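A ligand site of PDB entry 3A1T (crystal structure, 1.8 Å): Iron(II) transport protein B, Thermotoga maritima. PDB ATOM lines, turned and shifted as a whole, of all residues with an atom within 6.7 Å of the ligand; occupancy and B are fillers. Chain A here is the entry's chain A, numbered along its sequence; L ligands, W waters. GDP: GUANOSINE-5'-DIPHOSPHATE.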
ATOM      1  N   GLY A  12      26.046   8.984  -5.894  1.00  0.00           N
ATOM      2  CA  GLY A  12      26.449   9.957  -6.894  1.00  0.00           C
ATOM      3  C   GLY A  12      27.144  11.170  -6.315  1.00  0.00           C
ATOM      4  O   GLY A  12      27.034  11.463  -5.131  1.00  0.00           O
ATOM      5  N   CYS A  13      27.836  11.911  -7.179  1.00  0.00           N
ATOM      6  CA  CYS A  13      28.444  13.179  -6.778  1.00  0.00           C
ATOM      7  C   CYS A  13      27.339  14.157  -6.386  1.00  0.00           C
ATOM      8  O   CYS A  13      26.179  14.011  -6.829  1.00  0.00           O
ATOM      9  CB  CYS A  13      29.272  13.770  -7.915  1.00  0.00           C
ATOM     10  SG  CYS A  13      30.622  12.721  -8.494  1.00  0.00           S
ATOM     11  N   PRO A  14      27.678  15.152  -5.555  1.00  0.00           N
ATOM     12  CA  PRO A  14      26.743  16.238  -5.257  1.00  0.00           C
ATOM     13  C   PRO A  14      26.298  16.924  -6.549  1.00  0.00           C
ATOM     14  O   PRO A  14      27.090  17.022  -7.483  1.00  0.00           O
ATOM     15  CB  PRO A  14      27.578  17.225  -4.433  1.00  0.00           C
ATOM     16  CG  PRO A  14      28.679  16.410  -3.864  1.00  0.00           C
ATOM     17  CD  PRO A  14      28.973  15.345  -4.873  1.00  0.00           C
ATOM     18  N   ASN A  15      25.042  17.359  -6.584  1.00  0.00           N
ATOM     19  CA  ASN A  15      24.541  18.119  -7.721  1.00  0.00           C
ATOM     20  C   ASN A  15      24.620  17.467  -9.099  1.00  0.00           C
ATOM     21  O   ASN A  15      24.958  18.127 -10.084  1.00  0.00           O
ATOM     22  CB  ASN A  15      25.215  19.497  -7.753  1.00  0.00           C
ATOM     23  CG  ASN A  15      24.310  20.563  -7.215  1.00  0.00           C
ATOM     24  OD1 ASN A  15      23.360  20.980  -7.879  1.00  0.00           O
ATOM     25  ND2 ASN A  15      24.577  20.980  -5.983  1.00  0.00           N
ATOM     26  N   VAL A  16      24.307  16.188  -9.167  1.00  0.00           N
ATOM     27  CA  VAL A  16      24.279  15.549 -10.467  1.00  0.00           C
ATOM     28  C   VAL A  16      22.832  15.322 -10.894  1.00  0.00           C
ATOM     29  O   VAL A  16      22.571  15.055 -12.063  1.00  0.00           O
ATOM     30  CB  VAL A  16      25.030  14.197 -10.492  1.00  0.00           C
ATOM     31  CG1 VAL A  16      26.524  14.411 -10.242  1.00  0.00           C
ATOM     32  CG2 VAL A  16      24.425  13.248  -9.460  1.00  0.00           C
ATOM     33  N   GLY A  17      21.900  15.451  -9.961  1.00  0.00           N
ATOM     34  CA  GLY A  17      20.492  15.182 -10.247  1.00  0.00           C
ATOM     35  C   GLY A  17      19.926  13.969  -9.507  1.00  0.00           C
ATOM     36  O   GLY A  17      18.928  13.389  -9.932  1.00  0.00           O
ATOM     37  N   LYS A  18      20.550  13.580  -8.392  1.00  0.00           N
ATOM     38  CA  LYS A  18      20.066  12.455  -7.597  1.00  0.00           C
ATOM     39  C   LYS A  18      18.689  12.704  -6.995  1.00  0.00           C
ATOM     40  O   LYS A  18      17.817  11.853  -7.081  1.00  0.00           O
ATOM     41  CB  LYS A  18      21.046  12.104  -6.466  1.00  0.00           C
ATOM     42  CG  LYS A  18      22.129  11.126  -6.847  1.00  0.00           C
ATOM     43  CD  LYS A  18      22.485  10.197  -5.687  1.00  0.00           C
ATOM     44  CE  LYS A  18      23.216  10.937  -4.563  1.00  0.00           C
ATOM     45  NZ  LYS A  18      22.296  11.618  -3.608  1.00  0.00           N
ATOM     46  N   THR A  19      18.513  13.856  -6.356  1.00  0.00           N
ATOM     47  CA  THR A  19      17.258  14.156  -5.698  1.00  0.00           C
ATOM     48  C   THR A  19      16.107  14.128  -6.707  1.00  0.00           C
ATOM     49  O   THR A  19      15.031  13.579  -6.432  1.00  0.00           O
ATOM     50  CB  THR A  19      17.281  15.546  -5.039  1.00  0.00           C
ATOM     51  OG1 THR A  19      18.243  15.545  -3.980  1.00  0.00           O
ATOM     52  CG2 THR A  19      15.902  15.922  -4.487  1.00  0.00           C
ATOM     53  N   SER A  20      16.339  14.740  -7.858  1.00  0.00           N
ATOM     54  CA  SER A  20      15.300  14.800  -8.892  1.00  0.00           C
ATOM     55  C   SER A  20      14.919  13.387  -9.351  1.00  0.00           C
ATOM     56  O   SER A  20      13.734  13.073  -9.542  1.00  0.00           O
ATOM     57  CB  SER A  20      15.806  15.635 -10.082  1.00  0.00           C
ATOM     58  OG  SER A  20      16.060  16.978  -9.671  1.00  0.00           O
ATOM     59  N   LEU A  21      15.920  12.543  -9.537  1.00  0.00           N
ATOM     60  CA  LEU A  21      15.687  11.193 -10.001  1.00  0.00           C
ATOM     61  C   LEU A  21      14.973  10.385  -8.909  1.00  0.00           C
ATOM     62  O   LEU A  21      14.040   9.642  -9.189  1.00  0.00           O
ATOM     63  CB  LEU A  21      17.007  10.527 -10.426  1.00  0.00           C
ATOM     64  CG  LEU A  21      16.903   9.093 -10.959  1.00  0.00           C
ATOM     65  CD1 LEU A  21      15.992   9.024 -12.196  1.00  0.00           C
ATOM     66  CD2 LEU A  21      18.292   8.500 -11.268  1.00  0.00           C
ATOM     67  N   ASN A  23      12.985  11.614  -6.469  1.00  0.00           N
ATOM     68  CA  ASN A  23      11.597  12.080  -6.508  1.00  0.00           C
ATOM     69  C   ASN A  23      10.771  11.482  -7.666  1.00  0.00           C
ATOM     70  O   ASN A  23       9.608  11.143  -7.499  1.00  0.00           O
ATOM     71  CB  ASN A  23      11.542  13.620  -6.621  1.00  0.00           C
ATOM     72  CG  ASN A  23      11.993  14.321  -5.355  1.00  0.00           C
ATOM     73  OD1 ASN A  23      12.146  13.701  -4.295  1.00  0.00           O
ATOM     74  ND2 ASN A  23      12.189  15.629  -5.442  1.00  0.00           N
ATOM     75  N   LYS A  43      16.985   9.780   3.379  1.00  0.00           N
ATOM     76  CA  LYS A  43      15.778   9.693   2.561  1.00  0.00           C
ATOM     77  C   LYS A  43      15.569   8.302   1.995  1.00  0.00           C
ATOM     78  O   LYS A  43      16.457   7.726   1.392  1.00  0.00           O
ATOM     79  CB  LYS A  43      15.783  10.744   1.437  1.00  0.00           C
ATOM     80  CG  LYS A  43      15.247  12.088   1.873  1.00  0.00           C
ATOM     81  CD  LYS A  43      14.816  12.926   0.682  1.00  0.00           C
ATOM     82  CE  LYS A  43      15.954  13.081  -0.304  1.00  0.00           C
ATOM     83  NZ  LYS A  43      15.731  14.231  -1.216  1.00  0.00           N
ATOM     84  N   ASP A  58      18.340   7.123  -0.863  1.00  0.00           N
ATOM     85  CA  ASP A  58      19.196   8.132  -1.456  1.00  0.00           C
ATOM     86  C   ASP A  58      20.392   8.385  -0.525  1.00  0.00           C
ATOM     87  O   ASP A  58      20.210   8.820   0.614  1.00  0.00           O
ATOM     88  CB  ASP A  58      18.444   9.458  -1.626  1.00  0.00           C
ATOM     89  CG  ASP A  58      19.223  10.437  -2.479  1.00  0.00           C
ATOM     90  OD1 ASP A  58      20.076   9.979  -3.260  1.00  0.00           O
ATOM     91  OD2 ASP A  58      19.000  11.651  -2.369  1.00  0.00           O
ATOM     92  N   GLY A  61      25.405  12.845  -1.155  1.00  0.00           N
ATOM     93  CA  GLY A  61      26.282  13.070  -2.287  1.00  0.00           C
ATOM     94  C   GLY A  61      27.739  12.878  -1.898  1.00  0.00           C
ATOM     95  O   GLY A  61      28.115  13.241  -0.789  1.00  0.00           O
ATOM     96  N   VAL A  90      24.307   7.445 -10.083  1.00  0.00           N
ATOM     97  CA  VAL A  90      23.709   8.521 -10.848  1.00  0.00           C
ATOM     98  C   VAL A  90      24.798   9.467 -11.354  1.00  0.00           C
ATOM     99  O   VAL A  90      25.484  10.094 -10.555  1.00  0.00           O
ATOM    100  CB  VAL A  90      22.675   9.330 -10.027  1.00  0.00           C
ATOM    101  CG1 VAL A  90      22.026  10.382 -10.914  1.00  0.00           C
ATOM    102  CG2 VAL A  90      21.594   8.383  -9.437  1.00  0.00           C
ATOM    103  N   THR A 118      22.151  10.601 -16.114  1.00  0.00           N
ATOM    104  CA  THR A 118      20.988  11.474 -16.064  1.00  0.00           C
ATOM    105  C   THR A 118      21.254  12.813 -16.768  1.00  0.00           C
ATOM    106  O   THR A 118      22.336  13.023 -17.325  1.00  0.00           O
ATOM    107  CB  THR A 118      20.457  11.617 -14.630  1.00  0.00           C
ATOM    108  OG1 THR A 118      19.090  12.057 -14.661  1.00  0.00           O
ATOM    109  CG2 THR A 118      21.332  12.566 -13.759  1.00  0.00           C
ATOM    110  N   ALA A 119      20.263  13.690 -16.764  1.00  0.00           N
ATOM    111  CA  ALA A 119      20.315  14.926 -17.554  1.00  0.00           C
ATOM    112  C   ALA A 119      20.668  14.670 -19.020  1.00  0.00           C
ATOM    113  O   ALA A 119      21.296  15.487 -19.677  1.00  0.00           O
ATOM    114  CB  ALA A 119      21.276  15.954 -16.907  1.00  0.00           C
ATOM    115  N   ILE A 120      20.229  13.531 -19.547  1.00  0.00           N
ATOM    116  CA  ILE A 120      20.525  13.193 -20.928  1.00  0.00           C
ATOM    117  C   ILE A 120      19.884  14.206 -21.900  1.00  0.00           C
ATOM    118  O   ILE A 120      20.313  14.335 -23.044  1.00  0.00           O
ATOM    119  CB  ILE A 120      20.101  11.740 -21.274  1.00  0.00           C
ATOM    120  CG1 ILE A 120      20.904  11.201 -22.468  1.00  0.00           C
ATOM    121  CG2 ILE A 120      18.581  11.650 -21.546  1.00  0.00           C
ATOM    122  CD1 ILE A 120      22.394  11.041 -22.164  1.00  0.00           C
ATOM    123  N   ASP A 121      18.886  14.946 -21.423  1.00  0.00           N
ATOM    124  CA  ASP A 121      18.251  15.974 -22.249  1.00  0.00           C
ATOM    125  C   ASP A 121      19.188  17.137 -22.499  1.00  0.00           C
ATOM    126  O   ASP A 121      19.119  17.785 -23.534  1.00  0.00           O
ATOM    127  CB  ASP A 121      16.970  16.490 -21.587  1.00  0.00           C
ATOM    128  CG  ASP A 121      17.216  17.022 -20.183  1.00  0.00           C
ATOM    129  OD1 ASP A 121      17.677  16.232 -19.335  1.00  0.00           O
ATOM    130  OD2 ASP A 121      16.951  18.219 -19.932  1.00  0.00           O
ATOM    131  N   GLU A 122      20.073  17.418 -21.531  1.00  0.00           N
ATOM    132  CA  GLU A 122      21.011  18.515 -21.671  1.00  0.00           C
ATOM    133  C   GLU A 122      22.167  18.051 -22.573  1.00  0.00           C
ATOM    134  O   GLU A 122      22.728  18.846 -23.335  1.00  0.00           O
ATOM    135  CB  GLU A 122      21.500  18.997 -20.302  1.00  0.00           C
ATOM    136  CG  GLU A 122      22.500  20.165 -20.333  1.00  0.00           C
ATOM    137  CD  GLU A 122      21.888  21.488 -20.772  1.00  0.00           C
ATOM    138  OE1 GLU A 122      20.728  21.498 -21.221  1.00  0.00           O
ATOM    139  OE2 GLU A 122      22.567  22.523 -20.672  1.00  0.00           O
ATOM    140  N   THR A 146      18.834   8.634 -18.491  1.00  0.00           N
ATOM    141  CA  THR A 146      17.652   9.176 -17.822  1.00  0.00           C
ATOM    142  C   THR A 146      17.572  10.709 -17.891  1.00  0.00           C
ATOM    143  O   THR A 146      18.586  11.406 -18.055  1.00  0.00           O
ATOM    144  CB  THR A 146      17.573   8.753 -16.350  1.00  0.00           C
ATOM    145  OG1 THR A 146      18.638   9.378 -15.607  1.00  0.00           O
ATOM    146  CG2 THR A 146      17.682   7.242 -16.208  1.00  0.00           C
ATOM    147  N   SER A 147      16.352  11.228 -17.758  1.00  0.00           N
ATOM    148  CA  SER A 147      16.112  12.658 -17.607  1.00  0.00           C
ATOM    149  C   SER A 147      14.923  12.889 -16.687  1.00  0.00           C
ATOM    150  O   SER A 147      13.840  12.388 -16.942  1.00  0.00           O
ATOM    151  CB  SER A 147      15.802  13.323 -18.946  1.00  0.00           C
ATOM    152  OG  SER A 147      15.466  14.689 -18.728  1.00  0.00           O
ATOM    153  N   SER A 148      15.132  13.670 -15.634  1.00  0.00           N
ATOM    154  CA  SER A 148      14.035  14.022 -14.734  1.00  0.00           C
ATOM    155  C   SER A 148      13.205  15.135 -15.354  1.00  0.00           C
ATOM    156  O   SER A 148      12.078  15.398 -14.921  1.00  0.00           O
ATOM    157  CB  SER A 148      14.598  14.454 -13.371  1.00  0.00           C
ATOM    158  OG  SER A 148      15.221  13.366 -12.695  1.00  0.00           O
ATOM    159  N   VAL A 149      13.766  15.776 -16.369  1.00  0.00           N
ATOM    160  CA  VAL A 149      13.092  16.867 -17.077  1.00  0.00           C
ATOM    161  C   VAL A 149      12.100  16.306 -18.091  1.00  0.00           C
ATOM    162  O   VAL A 149      10.952  16.775 -18.177  1.00  0.00           O
ATOM    163  CB  VAL A 149      14.101  17.754 -17.810  1.00  0.00           C
ATOM    164  CG1 VAL A 149      13.395  18.681 -18.794  1.00  0.00           C
ATOM    165  CG2 VAL A 149      14.913  18.556 -16.797  1.00  0.00           C
ATOM    166  N   THR A 150      12.528  15.310 -18.862  1.00  0.00           N
ATOM    167  CA  THR A 150      11.705  14.787 -19.950  1.00  0.00           C
ATOM    168  C   THR A 150      11.039  13.454 -19.594  1.00  0.00           C
ATOM    169  O   THR A 150      10.089  13.043 -20.251  1.00  0.00           O
ATOM    170  CB  THR A 150      12.536  14.579 -21.222  1.00  0.00           C
ATOM    171  OG1 THR A 150      13.487  13.538 -21.005  1.00  0.00           O
ATOM    172  CG2 THR A 150      13.256  15.874 -21.625  1.00  0.00           C
HETATM  173  PB  GDP L   1      21.381  16.409  -6.407  1.00  0.00           P
HETATM  174  O1B GDP L   1      20.395  15.815  -5.424  1.00  0.00           O
HETATM  175  O2B GDP L   1      22.228  17.453  -5.706  1.00  0.00           O
HETATM  176  O3B GDP L   1      22.294  15.322  -6.908  1.00  0.00           O
HETATM  177  O3A GDP L   1      20.738  17.057  -7.727  1.00  0.00           O
HETATM  178  PA  GDP L   1      19.284  17.749  -7.928  1.00  0.00           P
HETATM  179  O1A GDP L   1      18.913  18.693  -6.809  1.00  0.00           O
HETATM  180  O2A GDP L   1      18.221  16.661  -8.103  1.00  0.00           O
HETATM  181  O5' GDP L   1      19.553  18.476  -9.313  1.00  0.00           O
HETATM  182  C5' GDP L   1      20.571  19.476  -9.403  1.00  0.00           C
HETATM  183  C4' GDP L   1      20.235  20.419 -10.541  1.00  0.00           C
HETATM  184  O4' GDP L   1      20.163  19.715 -11.786  1.00  0.00           O
HETATM  185  C3' GDP L   1      18.884  21.040 -10.323  1.00  0.00           C
HETATM  186  O3' GDP L   1      18.971  22.381 -10.791  1.00  0.00           O
HETATM  187  C2' GDP L   1      17.952  20.326 -11.278  1.00  0.00           C
HETATM  188  O2' GDP L   1      16.951  21.217 -11.751  1.00  0.00           O
HETATM  189  C1' GDP L   1      18.872  19.892 -12.398  1.00  0.00           C
HETATM  190  N9  GDP L   1      18.469  18.590 -12.988  1.00  0.00           N
HETATM  191  C8  GDP L   1      18.224  17.446 -12.316  1.00  0.00           C
HETATM  192  N7  GDP L   1      17.916  16.433 -13.167  1.00  0.00           N
HETATM  193  C5  GDP L   1      17.994  16.942 -14.412  1.00  0.00           C
HETATM  194  C6  GDP L   1      17.788  16.416 -15.771  1.00  0.00           C
HETATM  195  O6  GDP L   1      17.485  15.214 -15.916  1.00  0.00           O
HETATM  196  N1  GDP L   1      17.964  17.243 -16.808  1.00  0.00           N
HETATM  197  C2  GDP L   1      18.313  18.540 -16.644  1.00  0.00           C
HETATM  198  N2  GDP L   1      18.476  19.325 -17.739  1.00  0.00           N
HETATM  199  N3  GDP L   1      18.513  19.092 -15.417  1.00  0.00           N
HETATM  200  C4  GDP L   1      18.372  18.349 -14.287  1.00  0.00           C
HETATM  201  O   HOH W   1      20.870  14.118  -3.418  1.00  0.00           O
HETATM  202  O   HOH W   2      23.841  14.030  -5.197  1.00  0.00           O
HETATM  203  O   HOH W   3      14.669  20.755  -9.766  1.00  0.00           O
HETATM  204  O   HOH W   4      21.457  17.879  -2.816  1.00  0.00           O
HETATM  205  O   HOH W   5      17.950  13.641 -12.621  1.00  0.00           O
HETATM  206  O   HOH W   6      24.023  18.071  -3.620  1.00  0.00           O
HETATM  207  O   HOH W   7      19.868  19.921  -4.483  1.00  0.00           O
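The backbone NH (N) of Thr 19 lies within hydrogen-bond range of an oxygen (O1B) of the ligand (2.9 Å).
The side-chain hydroxyl (OG1) of Thr 19 lies within hydrogen-bond range of an oxygen (O1B) of the ligand (2.6 Å).
N of Ser 20 sits at hydrogen-bond distance from O2A of the ligand (2.7 Å).
O2A of the ligand is in hydrogen-bond range of OG of Ser 20, 2.7 Å away.
A nitrogen (N1) of the ligand sits at hydrogen-bond distance from the side-chain carboxylate (OD1) of Asp 121 (2.7 Å).
The backbone NH (N) of Ser 148 sits at hydrogen-bond distance from an oxygen (O6) of the ligand (2.8 Å).
An oxygen (O3B) of the ligand lies within hydrogen-bond range of the backbone NH of Lys 18 (2.9 Å).
The backbone NH (N) of Asn 15 sits at hydrogen-bond distance from an oxygen (O2B) of the ligand, 2.9 Å away.
N of Gly 17 is in hydrogen-bond range of O3A of the ligand.
N of Val 16 sits at hydrogen-bond distance from O3B of the ligand (3.1 Å).
The backbone NH of Ala 119 lies within hydrogen-bond range of an oxygen (O6) of the ligand, 3.3 Å away.
OG of Ser 148 lies close to O of Ser 20.
The side-chain carboxylate of Asp 121 is in hydrogen-bond range of the side-chain hydroxyl of Ser 147 (2.8 Å).
The side-chain hydroxyl (OG) of Ser 148 is in hydrogen-bond range of the backbone NH (N) of Leu 21, 3.3 Å away.
The side-chain carboxylate (OD1) of Asp 58 lies within salt-bridge range of the side-chain amino group (NZ) of Lys 18 (2.8 Å).
O of Thr 146 lies within hydrogen-bond range of N of Ala 119 (3.1 Å).
OG of Ser 147 sits at hydrogen-bond distance from N of Val 149, 3.1 Å away.
The backbone NH (N) of Thr 150 sits at hydrogen-bond distance from the side-chain hydroxyl (OG) of Ser 147, at 3.0 Å.
OG1 of Thr 146 is in hydrogen-bond range of OG1 of Thr 118.
Water W2 lies within hydrogen-bond range of O3B of the ligand (2.6 Å), O of Cys 13 (2.9 Å) and NZ of Lys 18 (3.3 Å).
Water W1 lies within hydrogen-bond range of an oxygen (O1B) of the ligand (2.7 Å), the side-chain amino group (NZ) of Lys 18 (2.9 Å), the side-chain hydroxyl (OG1) of Thr 19 (3.0 Å) and the side-chain carboxylate (OD2) of Asp 58 (3.3 Å).
Water W6 lies within hydrogen-bond range of O2B of the ligand (2.8 Å) and N of Asn 15 (3.2 Å).
Water W5 lies within hydrogen-bond range of the side-chain hydroxyl (OG) of Ser 148 (2.7 Å), the side-chain hydroxyl (OG1) of Thr 118 (2.8 Å), a nitrogen (N7) of the ligand (2.8 Å) and the backbone carbonyl oxygen (O) of Gly 17 (2.9 Å).
OG1 of Thr 118 touches O6 of the ligand (3.8 Å).
CB of Glu 122 touches N2 of the ligand, 3.98 Å away.
Ser 147 touches the ligand (CA to O6, 3.4 Å).
Val 149 touches the ligand.
The nearest printed residue that does not touch the ligand is Cys 13 (4.1 Å).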
